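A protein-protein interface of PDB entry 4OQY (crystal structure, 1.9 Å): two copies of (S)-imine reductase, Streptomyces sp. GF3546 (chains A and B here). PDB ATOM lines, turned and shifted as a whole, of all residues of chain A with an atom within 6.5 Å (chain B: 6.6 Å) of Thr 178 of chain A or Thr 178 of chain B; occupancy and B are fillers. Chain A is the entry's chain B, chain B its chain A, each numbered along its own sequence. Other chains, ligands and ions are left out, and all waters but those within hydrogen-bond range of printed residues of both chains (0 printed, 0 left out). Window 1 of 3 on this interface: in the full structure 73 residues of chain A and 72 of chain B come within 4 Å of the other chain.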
ATOM      1  N   MET A 173       3.960  20.237  12.769  1.00  0.00           N
ATOM      2  CA  MET A 173       4.286  19.476  13.959  1.00  0.00           C
ATOM      3  C   MET A 173       3.175  18.481  14.294  1.00  0.00           C
ATOM      4  O   MET A 173       3.464  17.437  14.846  1.00  0.00           O
ATOM      5  CB  MET A 173       4.643  20.398  15.124  1.00  0.00           C
ATOM      6  CG  MET A 173       5.884  21.251  14.871  1.00  0.00           C
ATOM      7  SD  MET A 173       7.277  20.368  14.152  1.00  0.00           S
ATOM      8  CE  MET A 173       7.708  19.393  15.597  1.00  0.00           C
ATOM      9  N   THR A 174       1.931  18.766  13.900  1.00  0.00           N
ATOM     10  CA  THR A 174       0.836  17.798  14.047  1.00  0.00           C
ATOM     11  C   THR A 174       1.141  16.484  13.312  1.00  0.00           C
ATOM     12  O   THR A 174       1.062  15.375  13.868  1.00  0.00           O
ATOM     13  CB  THR A 174      -0.506  18.384  13.510  1.00  0.00           C
ATOM     14  OG1 THR A 174      -0.827  19.600  14.198  1.00  0.00           O
ATOM     15  CG2 THR A 174      -1.632  17.394  13.667  1.00  0.00           C
ATOM     16  N   ILE A 175       1.499  16.625  12.053  1.00  0.00           N
ATOM     17  CA  ILE A 175       1.868  15.495  11.229  1.00  0.00           C
ATOM     18  C   ILE A 175       3.140  14.826  11.741  1.00  0.00           C
ATOM     19  O   ILE A 175       3.210  13.598  11.805  1.00  0.00           O
ATOM     20  CB  ILE A 175       2.043  15.940   9.774  1.00  0.00           C
ATOM     21  CG1 ILE A 175       0.690  16.383   9.220  1.00  0.00           C
ATOM     22  CG2 ILE A 175       2.662  14.829   8.932  1.00  0.00           C
ATOM     23  CD1 ILE A 175       0.783  17.152   7.916  1.00  0.00           C
ATOM     24  N   PHE A 176       4.147  15.617  12.101  1.00  0.00           N
ATOM     25  CA  PHE A 176       5.422  15.062  12.554  1.00  0.00           C
ATOM     26  C   PHE A 176       5.283  14.215  13.809  1.00  0.00           C
ATOM     27  O   PHE A 176       5.708  13.062  13.830  1.00  0.00           O
ATOM     28  CB  PHE A 176       6.432  16.148  12.843  1.00  0.00           C
ATOM     29  CG  PHE A 176       7.752  15.611  13.217  1.00  0.00           C
ATOM     30  CD1 PHE A 176       8.601  15.131  12.228  1.00  0.00           C
ATOM     31  CD2 PHE A 176       8.156  15.539  14.525  1.00  0.00           C
ATOM     32  CE1 PHE A 176       9.828  14.598  12.555  1.00  0.00           C
ATOM     33  CE2 PHE A 176       9.402  15.020  14.847  1.00  0.00           C
ATOM     34  CZ  PHE A 176      10.230  14.547  13.864  1.00  0.00           C
ATOM     35  N   TRP A 177       4.662  14.779  14.855  1.00  0.00           N
ATOM     36  CA  TRP A 177       4.549  14.053  16.121  1.00  0.00           C
ATOM     37  C   TRP A 177       3.602  12.857  16.037  1.00  0.00           C
ATOM     38  O   TRP A 177       3.868  11.814  16.621  1.00  0.00           O
ATOM     39  CB  TRP A 177       4.119  14.968  17.260  1.00  0.00           C
ATOM     40  CG  TRP A 177       5.115  16.017  17.647  1.00  0.00           C
ATOM     41  CD1 TRP A 177       4.879  17.347  17.720  1.00  0.00           C
ATOM     42  CD2 TRP A 177       6.496  15.833  18.036  1.00  0.00           C
ATOM     43  NE1 TRP A 177       6.009  18.012  18.118  1.00  0.00           N
ATOM     44  CE2 TRP A 177       7.018  17.109  18.318  1.00  0.00           C
ATOM     45  CE3 TRP A 177       7.322  14.721  18.203  1.00  0.00           C
ATOM     46  CZ2 TRP A 177       8.333  17.306  18.746  1.00  0.00           C
ATOM     47  CZ3 TRP A 177       8.623  14.915  18.628  1.00  0.00           C
ATOM     48  CH2 TRP A 177       9.117  16.201  18.894  1.00  0.00           C
ATOM     49  N   THR A 178       2.502  13.016  15.317  1.00  0.00           N
ATOM     50  CA  THR A 178       1.573  11.923  15.146  1.00  0.00           C
ATOM     51  C   THR A 178       2.230  10.763  14.390  1.00  0.00           C
ATOM     52  O   THR A 178       2.073   9.607  14.754  1.00  0.00           O
ATOM     53  CB  THR A 178       0.268  12.397  14.475  1.00  0.00           C
ATOM     54  OG1 THR A 178      -0.258  13.510  15.207  1.00  0.00           O
ATOM     55  CG2 THR A 178      -0.749  11.302  14.477  1.00  0.00           C
ATOM     56  N   THR A 179       2.980  11.074  13.350  1.00  0.00           N
ATOM     57  CA  THR A 179       3.632  10.047  12.574  1.00  0.00           C
ATOM     58  C   THR A 179       4.706   9.378  13.407  1.00  0.00           C
ATOM     59  O   THR A 179       4.830   8.154  13.417  1.00  0.00           O
ATOM     60  CB  THR A 179       4.242  10.650  11.317  1.00  0.00           C
ATOM     61  OG1 THR A 179       3.206  11.287  10.576  1.00  0.00           O
ATOM     62  CG2 THR A 179       4.885   9.580  10.473  1.00  0.00           C
ATOM     63  N   MET A 180       5.447  10.193  14.140  1.00  0.00           N
ATOM     64  CA  MET A 180       6.453   9.669  15.032  1.00  0.00           C
ATOM     65  C   MET A 180       5.839   8.681  16.030  1.00  0.00           C
ATOM     66  O   MET A 180       6.386   7.609  16.254  1.00  0.00           O
ATOM     67  CB  MET A 180       7.182  10.794  15.760  1.00  0.00           C
ATOM     68  CG  MET A 180       8.025  10.302  16.919  1.00  0.00           C
ATOM     69  SD  MET A 180       9.223  11.506  17.538  1.00  0.00           S
ATOM     70  CE  MET A 180       8.973  11.373  19.281  1.00  0.00           C
ATOM     71  N   LEU A 181       4.698   9.001  16.627  1.00  0.00           N
ATOM     72  CA  LEU A 181       4.116   8.042  17.551  1.00  0.00           C
ATOM     73  C   LEU A 181       3.659   6.772  16.846  1.00  0.00           C
ATOM     74  O   LEU A 181       3.760   5.712  17.412  1.00  0.00           O
ATOM     75  CB  LEU A 181       2.968   8.654  18.390  1.00  0.00           C
ATOM     76  CG  LEU A 181       3.397   9.677  19.449  1.00  0.00           C
ATOM     77  CD1 LEU A 181       2.233  10.107  20.349  1.00  0.00           C
ATOM     78  CD2 LEU A 181       4.521   9.131  20.313  1.00  0.00           C
ATOM     79  N   SER A 182       3.149   6.868  15.627  1.00  0.00           N
ATOM     80  CA  SER A 182       2.671   5.674  14.929  1.00  0.00           C
ATOM     81  C   SER A 182       3.848   4.736  14.626  1.00  0.00           C
ATOM     82  O   SER A 182       3.720   3.518  14.643  1.00  0.00           O
ATOM     83  CB  SER A 182       1.924   6.047  13.658  1.00  0.00           C
ATOM     84  OG  SER A 182       2.786   6.432  12.611  1.00  0.00           O
ATOM     85  N   TYR A 183       4.995   5.350  14.400  1.00  0.00           N
ATOM     86  CA  TYR A 183       6.250   4.642  14.159  1.00  0.00           C
ATOM     87  C   TYR A 183       6.646   3.884  15.417  1.00  0.00           C
ATOM     88  O   TYR A 183       6.795   2.670  15.404  1.00  0.00           O
ATOM     89  CB  TYR A 183       7.273   5.685  13.782  1.00  0.00           C
ATOM     90  CG  TYR A 183       8.667   5.227  13.589  1.00  0.00           C
ATOM     91  CD1 TYR A 183       9.034   4.682  12.386  1.00  0.00           C
ATOM     92  CD2 TYR A 183       9.642   5.399  14.574  1.00  0.00           C
ATOM     93  CE1 TYR A 183      10.331   4.293  12.146  1.00  0.00           C
ATOM     94  CE2 TYR A 183      10.961   4.999  14.342  1.00  0.00           C
ATOM     95  CZ  TYR A 183      11.278   4.441  13.125  1.00  0.00           C
ATOM     96  OH  TYR A 183      12.565   4.016  12.827  1.00  0.00           O
ATOM     97  N   VAL A 244      -6.537  -2.950  12.545  1.00  0.00           N
ATOM     98  CA  VAL A 244      -5.422  -2.294  13.234  1.00  0.00           C
ATOM     99  C   VAL A 244      -5.689  -2.213  14.755  1.00  0.00           C
ATOM    100  O   VAL A 244      -4.874  -2.613  15.568  1.00  0.00           O
ATOM    101  CB  VAL A 244      -5.137  -0.887  12.643  1.00  0.00           C
ATOM    102  CG1 VAL A 244      -4.183  -0.102  13.539  1.00  0.00           C
ATOM    103  CG2 VAL A 244      -4.541  -0.990  11.231  1.00  0.00           C
ATOM    104  N   LEU A 257      -3.472   5.485  20.819  1.00  0.00           N
ATOM    105  CA  LEU A 257      -3.399   5.996  19.477  1.00  0.00           C
ATOM    106  C   LEU A 257      -4.321   5.281  18.456  1.00  0.00           C
ATOM    107  O   LEU A 257      -5.123   5.932  17.795  1.00  0.00           O
ATOM    108  CB  LEU A 257      -1.939   5.994  19.011  1.00  0.00           C
ATOM    109  CG  LEU A 257      -1.697   6.642  17.664  1.00  0.00           C
ATOM    110  CD1 LEU A 257      -2.020   8.129  17.717  1.00  0.00           C
ATOM    111  CD2 LEU A 257      -0.245   6.400  17.263  1.00  0.00           C
ATOM    112  N   PRO A 258      -4.203   3.954  18.304  1.00  0.00           N
ATOM    113  CA  PRO A 258      -5.156   3.332  17.378  1.00  0.00           C
ATOM    114  C   PRO A 258      -6.637   3.498  17.817  1.00  0.00           C
ATOM    115  O   PRO A 258      -7.513   3.518  16.969  1.00  0.00           O
ATOM    116  CB  PRO A 258      -4.760   1.862  17.364  1.00  0.00           C
ATOM    117  CG  PRO A 258      -3.867   1.656  18.532  1.00  0.00           C
ATOM    118  CD  PRO A 258      -3.297   2.983  18.935  1.00  0.00           C
ATOM    119  N   VAL A 261      -7.672   6.839  16.334  1.00  0.00           N
ATOM    120  CA  VAL A 261      -7.916   6.705  14.927  1.00  0.00           C
ATOM    121  C   VAL A 261      -9.264   6.031  14.624  1.00  0.00           C
ATOM    122  O   VAL A 261     -10.012   6.465  13.759  1.00  0.00           O
ATOM    123  CB  VAL A 261      -6.752   5.908  14.271  1.00  0.00           C
ATOM    124  CG1 VAL A 261      -7.081   5.581  12.835  1.00  0.00           C
ATOM    125  CG2 VAL A 261      -5.460   6.693  14.415  1.00  0.00           C
ATOM    126  N   MET B 173      -0.290  -0.575   8.049  1.00  0.00           N
ATOM    127  CA  MET B 173      -1.573   0.133   8.069  1.00  0.00           C
ATOM    128  C   MET B 173      -1.723   1.057   9.288  1.00  0.00           C
ATOM    129  O   MET B 173      -2.383   2.081   9.190  1.00  0.00           O
ATOM    130  CB  MET B 173      -2.741  -0.852   7.922  1.00  0.00           C
ATOM    131  CG  MET B 173      -2.716  -1.616   6.592  1.00  0.00           C
ATOM    132  SD  MET B 173      -2.372  -0.583   5.147  1.00  0.00           S
ATOM    133  CE  MET B 173      -3.901   0.335   5.087  1.00  0.00           C
ATOM    134  N   THR B 174      -1.061   0.740  10.394  1.00  0.00           N
ATOM    135  CA  THR B 174      -1.025   1.608  11.575  1.00  0.00           C
ATOM    136  C   THR B 174      -0.456   2.996  11.210  1.00  0.00           C
ATOM    137  O   THR B 174      -1.024   4.049  11.501  1.00  0.00           O
ATOM    138  CB  THR B 174      -0.176   0.977  12.707  1.00  0.00           C
ATOM    139  OG1 THR B 174      -0.706  -0.301  13.084  1.00  0.00           O
ATOM    140  CG2 THR B 174      -0.138   1.881  13.909  1.00  0.00           C
ATOM    141  N   ILE B 175       0.694   2.965  10.581  1.00  0.00           N
ATOM    142  CA  ILE B 175       1.373   4.171  10.146  1.00  0.00           C
ATOM    143  C   ILE B 175       0.611   4.897   9.064  1.00  0.00           C
ATOM    144  O   ILE B 175       0.489   6.124   9.118  1.00  0.00           O
ATOM    145  CB  ILE B 175       2.797   3.823   9.632  1.00  0.00           C
ATOM    146  CG1 ILE B 175       3.650   3.312  10.793  1.00  0.00           C
ATOM    147  CG2 ILE B 175       3.440   5.037   8.969  1.00  0.00           C
ATOM    148  CD1 ILE B 175       4.964   2.649  10.358  1.00  0.00           C
ATOM    149  N   PHE B 176       0.085   4.149   8.099  1.00  0.00           N
ATOM    150  CA  PHE B 176      -0.640   4.757   7.009  1.00  0.00           C
ATOM    151  C   PHE B 176      -1.884   5.513   7.494  1.00  0.00           C
ATOM    152  O   PHE B 176      -2.049   6.693   7.198  1.00  0.00           O
ATOM    153  CB  PHE B 176      -1.087   3.722   5.999  1.00  0.00           C
ATOM    154  CG  PHE B 176      -1.732   4.323   4.804  1.00  0.00           C
ATOM    155  CD1 PHE B 176      -0.965   4.930   3.831  1.00  0.00           C
ATOM    156  CD2 PHE B 176      -3.098   4.297   4.654  1.00  0.00           C
ATOM    157  CE1 PHE B 176      -1.551   5.505   2.720  1.00  0.00           C
ATOM    158  CE2 PHE B 176      -3.687   4.876   3.546  1.00  0.00           C
ATOM    159  CZ  PHE B 176      -2.912   5.469   2.576  1.00  0.00           C
ATOM    160  N   TRP B 177      -2.741   4.830   8.227  1.00  0.00           N
ATOM    161  CA  TRP B 177      -4.017   5.463   8.654  1.00  0.00           C
ATOM    162  C   TRP B 177      -3.810   6.596   9.658  1.00  0.00           C
ATOM    163  O   TRP B 177      -4.505   7.633   9.612  1.00  0.00           O
ATOM    164  CB  TRP B 177      -4.974   4.446   9.236  1.00  0.00           C
ATOM    165  CG  TRP B 177      -5.499   3.438   8.277  1.00  0.00           C
ATOM    166  CD1 TRP B 177      -5.453   2.090   8.434  1.00  0.00           C
ATOM    167  CD2 TRP B 177      -6.163   3.670   7.021  1.00  0.00           C
ATOM    168  NE1 TRP B 177      -6.038   1.462   7.368  1.00  0.00           N
ATOM    169  CE2 TRP B 177      -6.500   2.406   6.491  1.00  0.00           C
ATOM    170  CE3 TRP B 177      -6.547   4.812   6.319  1.00  0.00           C
ATOM    171  CZ2 TRP B 177      -7.165   2.251   5.263  1.00  0.00           C
ATOM    172  CZ3 TRP B 177      -7.224   4.653   5.106  1.00  0.00           C
ATOM    173  CH2 TRP B 177      -7.527   3.385   4.598  1.00  0.00           C
ATOM    174  N   THR B 178      -2.887   6.392  10.587  1.00  0.00           N
ATOM    175  CA  THR B 178      -2.579   7.418  11.561  1.00  0.00           C
ATOM    176  C   THR B 178      -1.999   8.663  10.896  1.00  0.00           C
ATOM    177  O   THR B 178      -2.388   9.780  11.201  1.00  0.00           O
ATOM    178  CB  THR B 178      -1.648   6.892  12.676  1.00  0.00           C
ATOM    179  OG1 THR B 178      -2.196   5.702  13.255  1.00  0.00           O
ATOM    180  CG2 THR B 178      -1.474   7.926  13.760  1.00  0.00           C
ATOM    181  N   THR B 179      -1.087   8.486   9.942  1.00  0.00           N
ATOM    182  CA  THR B 179      -0.536   9.623   9.268  1.00  0.00           C
ATOM    183  C   THR B 179      -1.627  10.317   8.454  1.00  0.00           C
ATOM    184  O   THR B 179      -1.720  11.556   8.412  1.00  0.00           O
ATOM    185  CB  THR B 179       0.606   9.155   8.369  1.00  0.00           C
ATOM    186  OG1 THR B 179       1.570   8.504   9.207  1.00  0.00           O
ATOM    187  CG2 THR B 179       1.222  10.312   7.684  1.00  0.00           C
ATOM    188  N   MET B 180      -2.452   9.514   7.802  1.00  0.00           N
ATOM    189  CA  MET B 180      -3.546  10.051   7.017  1.00  0.00           C
ATOM    190  C   MET B 180      -4.453  10.942   7.868  1.00  0.00           C
ATOM    191  O   MET B 180      -4.828  12.024   7.434  1.00  0.00           O
ATOM    192  CB  MET B 180      -4.352   8.934   6.342  1.00  0.00           C
ATOM    193  CG  MET B 180      -5.659   9.435   5.749  1.00  0.00           C
ATOM    194  SD  MET B 180      -6.715   8.269   4.885  1.00  0.00           S
ATOM    195  CE  MET B 180      -5.924   8.019   3.304  1.00  0.00           C
ATOM    196  N   LEU B 181      -4.799  10.510   9.069  1.00  0.00           N
ATOM    197  CA  LEU B 181      -5.674  11.373   9.899  1.00  0.00           C
ATOM    198  C   LEU B 181      -4.959  12.661  10.314  1.00  0.00           C
ATOM    199  O   LEU B 181      -5.564  13.692  10.370  1.00  0.00           O
ATOM    200  CB  LEU B 181      -6.190  10.635  11.119  1.00  0.00           C
ATOM    201  CG  LEU B 181      -7.249   9.572  10.820  1.00  0.00           C
ATOM    202  CD1 LEU B 181      -7.882   9.026  12.107  1.00  0.00           C
ATOM    203  CD2 LEU B 181      -8.357  10.134   9.939  1.00  0.00           C
ATOM    204  N   SER B 182      -3.649  12.608  10.550  1.00  0.00           N
ATOM    205  CA  SER B 182      -2.942  13.813  10.965  1.00  0.00           C
ATOM    206  C   SER B 182      -2.938  14.838   9.825  1.00  0.00           C
ATOM    207  O   SER B 182      -2.958  16.048  10.031  1.00  0.00           O
ATOM    208  CB  SER B 182      -1.512  13.477  11.428  1.00  0.00           C
ATOM    209  OG  SER B 182      -0.651  13.189  10.347  1.00  0.00           O
ATOM    210  N   TYR B 183      -2.892  14.315   8.609  1.00  0.00           N
ATOM    211  CA  TYR B 183      -2.929  15.119   7.414  1.00  0.00           C
ATOM    212  C   TYR B 183      -4.296  15.830   7.343  1.00  0.00           C
ATOM    213  O   TYR B 183      -4.382  17.041   7.204  1.00  0.00           O
ATOM    214  CB  TYR B 183      -2.681  14.183   6.241  1.00  0.00           C
ATOM    215  CG  TYR B 183      -2.923  14.761   4.900  1.00  0.00           C
ATOM    216  CD1 TYR B 183      -4.141  14.581   4.296  1.00  0.00           C
ATOM    217  CD2 TYR B 183      -1.931  15.440   4.206  1.00  0.00           C
ATOM    218  CE1 TYR B 183      -4.402  15.073   3.044  1.00  0.00           C
ATOM    219  CE2 TYR B 183      -2.183  15.946   2.943  1.00  0.00           C
ATOM    220  CZ  TYR B 183      -3.439  15.755   2.390  1.00  0.00           C
ATOM    221  OH  TYR B 183      -3.743  16.234   1.159  1.00  0.00           O
ATOM    222  N   VAL B 244       0.882  22.068  19.935  1.00  0.00           N
ATOM    223  CA  VAL B 244       0.014  21.434  18.928  1.00  0.00           C
ATOM    224  C   VAL B 244      -1.418  21.293  19.504  1.00  0.00           C
ATOM    225  O   VAL B 244      -2.381  21.718  18.878  1.00  0.00           O
ATOM    226  CB  VAL B 244       0.558  20.067  18.449  1.00  0.00           C
ATOM    227  CG1 VAL B 244      -0.479  19.291  17.650  1.00  0.00           C
ATOM    228  CG2 VAL B 244       1.807  20.257  17.595  1.00  0.00           C
ATOM    229  N   LEU B 257      -7.412  13.328  18.051  1.00  0.00           N
ATOM    230  CA  LEU B 257      -6.068  12.893  17.683  1.00  0.00           C
ATOM    231  C   LEU B 257      -4.934  13.634  18.426  1.00  0.00           C
ATOM    232  O   LEU B 257      -4.091  12.990  19.055  1.00  0.00           O
ATOM    233  CB  LEU B 257      -5.905  12.971  16.176  1.00  0.00           C
ATOM    234  CG  LEU B 257      -4.589  12.402  15.644  1.00  0.00           C
ATOM    235  CD1 LEU B 257      -4.500  10.911  15.908  1.00  0.00           C
ATOM    236  CD2 LEU B 257      -4.515  12.701  14.150  1.00  0.00           C
ATOM    237  N   PRO B 258      -4.898  14.979  18.374  1.00  0.00           N
ATOM    238  CA  PRO B 258      -3.820  15.622  19.147  1.00  0.00           C
ATOM    239  C   PRO B 258      -3.921  15.381  20.655  1.00  0.00           C
ATOM    240  O   PRO B 258      -2.906  15.356  21.336  1.00  0.00           O
ATOM    241  CB  PRO B 258      -3.976  17.110  18.841  1.00  0.00           C
ATOM    242  CG  PRO B 258      -5.304  17.286  18.208  1.00  0.00           C
ATOM    243  CD  PRO B 258      -5.744  15.955  17.662  1.00  0.00           C
ATOM    244  N   VAL B 261      -2.074  12.052  21.177  1.00  0.00           N
ATOM    245  CA  VAL B 261      -0.643  12.255  21.106  1.00  0.00           C
ATOM    246  C   VAL B 261      -0.120  12.873  22.423  1.00  0.00           C
ATOM    247  O   VAL B 261       0.892  12.443  22.959  1.00  0.00           O
ATOM    248  CB  VAL B 261      -0.299  13.136  19.895  1.00  0.00           C
ATOM    249  CG1 VAL B 261       1.157  13.536  19.945  1.00  0.00           C
ATOM    250  CG2 VAL B 261      -0.670  12.407  18.612  1.00  0.00           C
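Hydrophobic or aromatic side chains of chain B that line the printed part of chain A: Met 173, Ile 175, Leu 181, Val 244 and Val 261. Of the 15 printed residues of chain A, 10 touch a printed residue of chain B. Hydrophobic or aromatic side chains of chain A that line the printed part of chain B: Met 173, Ile 175, Leu 181, Val 244, Leu 257 and Val 261. Among the printed residues, 15 pairs touch across the chains.
Thr 178 of chain A touches Ser 182 of chain B, and with the chains exchanged Ser 182 of chain A touches Thr 178 of chain B. Thr 178 of chain A touches Val 261 of chain B, and with the chains exchanged Val 261 of chain A touches Thr 178 of chain B. Thr 179 of chain A touches its own counterpart, Thr 179 of chain B. Leu 181 of chain A touches Val 261 of chain B, and with the chains exchanged Val 261 of chain A touches Leu 181 of chain B.
Among the printed residues, pairs that only touch across the chains: Thr 174 of chain A with Val 244 of chain B (3.5 Å), Thr 179 of chain A with Thr 179 of chain B (3.5 Å), Val 244 of chain A with Thr 174 of chain B (3.5 Å), Thr 178 of chain A with Thr 178 of chain B (3.5 Å), Ile 175 of chain A with Ser 182 of chain B (3.5 Å), Thr 178 of chain A with Val 261 of chain B (3.6 Å), Val 261 of chain A with Thr 178 of chain B (3.6 Å), Val 261 of chain A with Leu 181 of chain B (3.6 Å), Leu 181 of chain A with Val 261 of chain B (3.6 Å), Ser 182 of chain A with Ile 175 of chain B (3.6 Å), Thr 178 of chain A with Ser 182 of chain B (3.7 Å), Met 173 of chain A with Val 244 of chain B (3.8 Å), Val 244 of chain A with Met 173 of chain B (3.8 Å), Ser 182 of chain A with Thr 178 of chain B (3.8 Å) and Leu 257 of chain A with Thr 178 of chain B (3.9996 Å).
O of Thr 179 of chain B sits at hydrogen-bond distance from OG of Ser 182 of chain B (2.7 Å). O of Ile 175 of chain B lies within hydrogen-bond range of OG1 of Thr 179 of chain B, 2.6 Å away. OG of Ser 182 of chain A lies within hydrogen-bond range of O of Thr 179 of chain A (2.8 Å). The backbone carbonyl oxygen (O) of Thr 174 of chain A lies within hydrogen-bond range of the side-chain hydroxyl (OG1) of Thr 178 of chain A. The side-chain hydroxyl of Thr 178 of chain B lies within hydrogen-bond range of the backbone carbonyl oxygen of Thr 174 of chain B. O of Ile 175 of chain A is in hydrogen-bond range of OG1 of Thr 179 of chain A.
Thr 178 of chain A touches three residues of chain B. Of the printed residues of chain B, Thr 179 of chain A touches Thr 179. Printed residues of chain B within 4 Å of Val 244 of chain A: Met 173 (3.8 Å) and Thr 174 (3.5 Å). Of the printed residues of chain A, Met 173 of chain B touches Val 244 (3.8 Å). Printed residues of chain A within 4 Å of Ile 175 of chain B: Ser 182 (3.6 Å). Phe 176 of chain B touches none of the printed residues of chain A. Printed residues of chain A within 4 Å of Thr 178 of chain B: Thr 178 (3.5 Å), Ser 182 (3.8 Å), Leu 257 (3.9996 Å) and Val 261 (3.6 Å). Pro 258 of chain B touches none of the printed residues of chain A. The nearest residue of chain B that does not touch Thr 178 of chain A is Leu 257 of chain B (4.03 Å). The nearest printed residue of chain A that does not touch Thr 178 of chain B is Thr 179 of chain A (5.5 Å).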
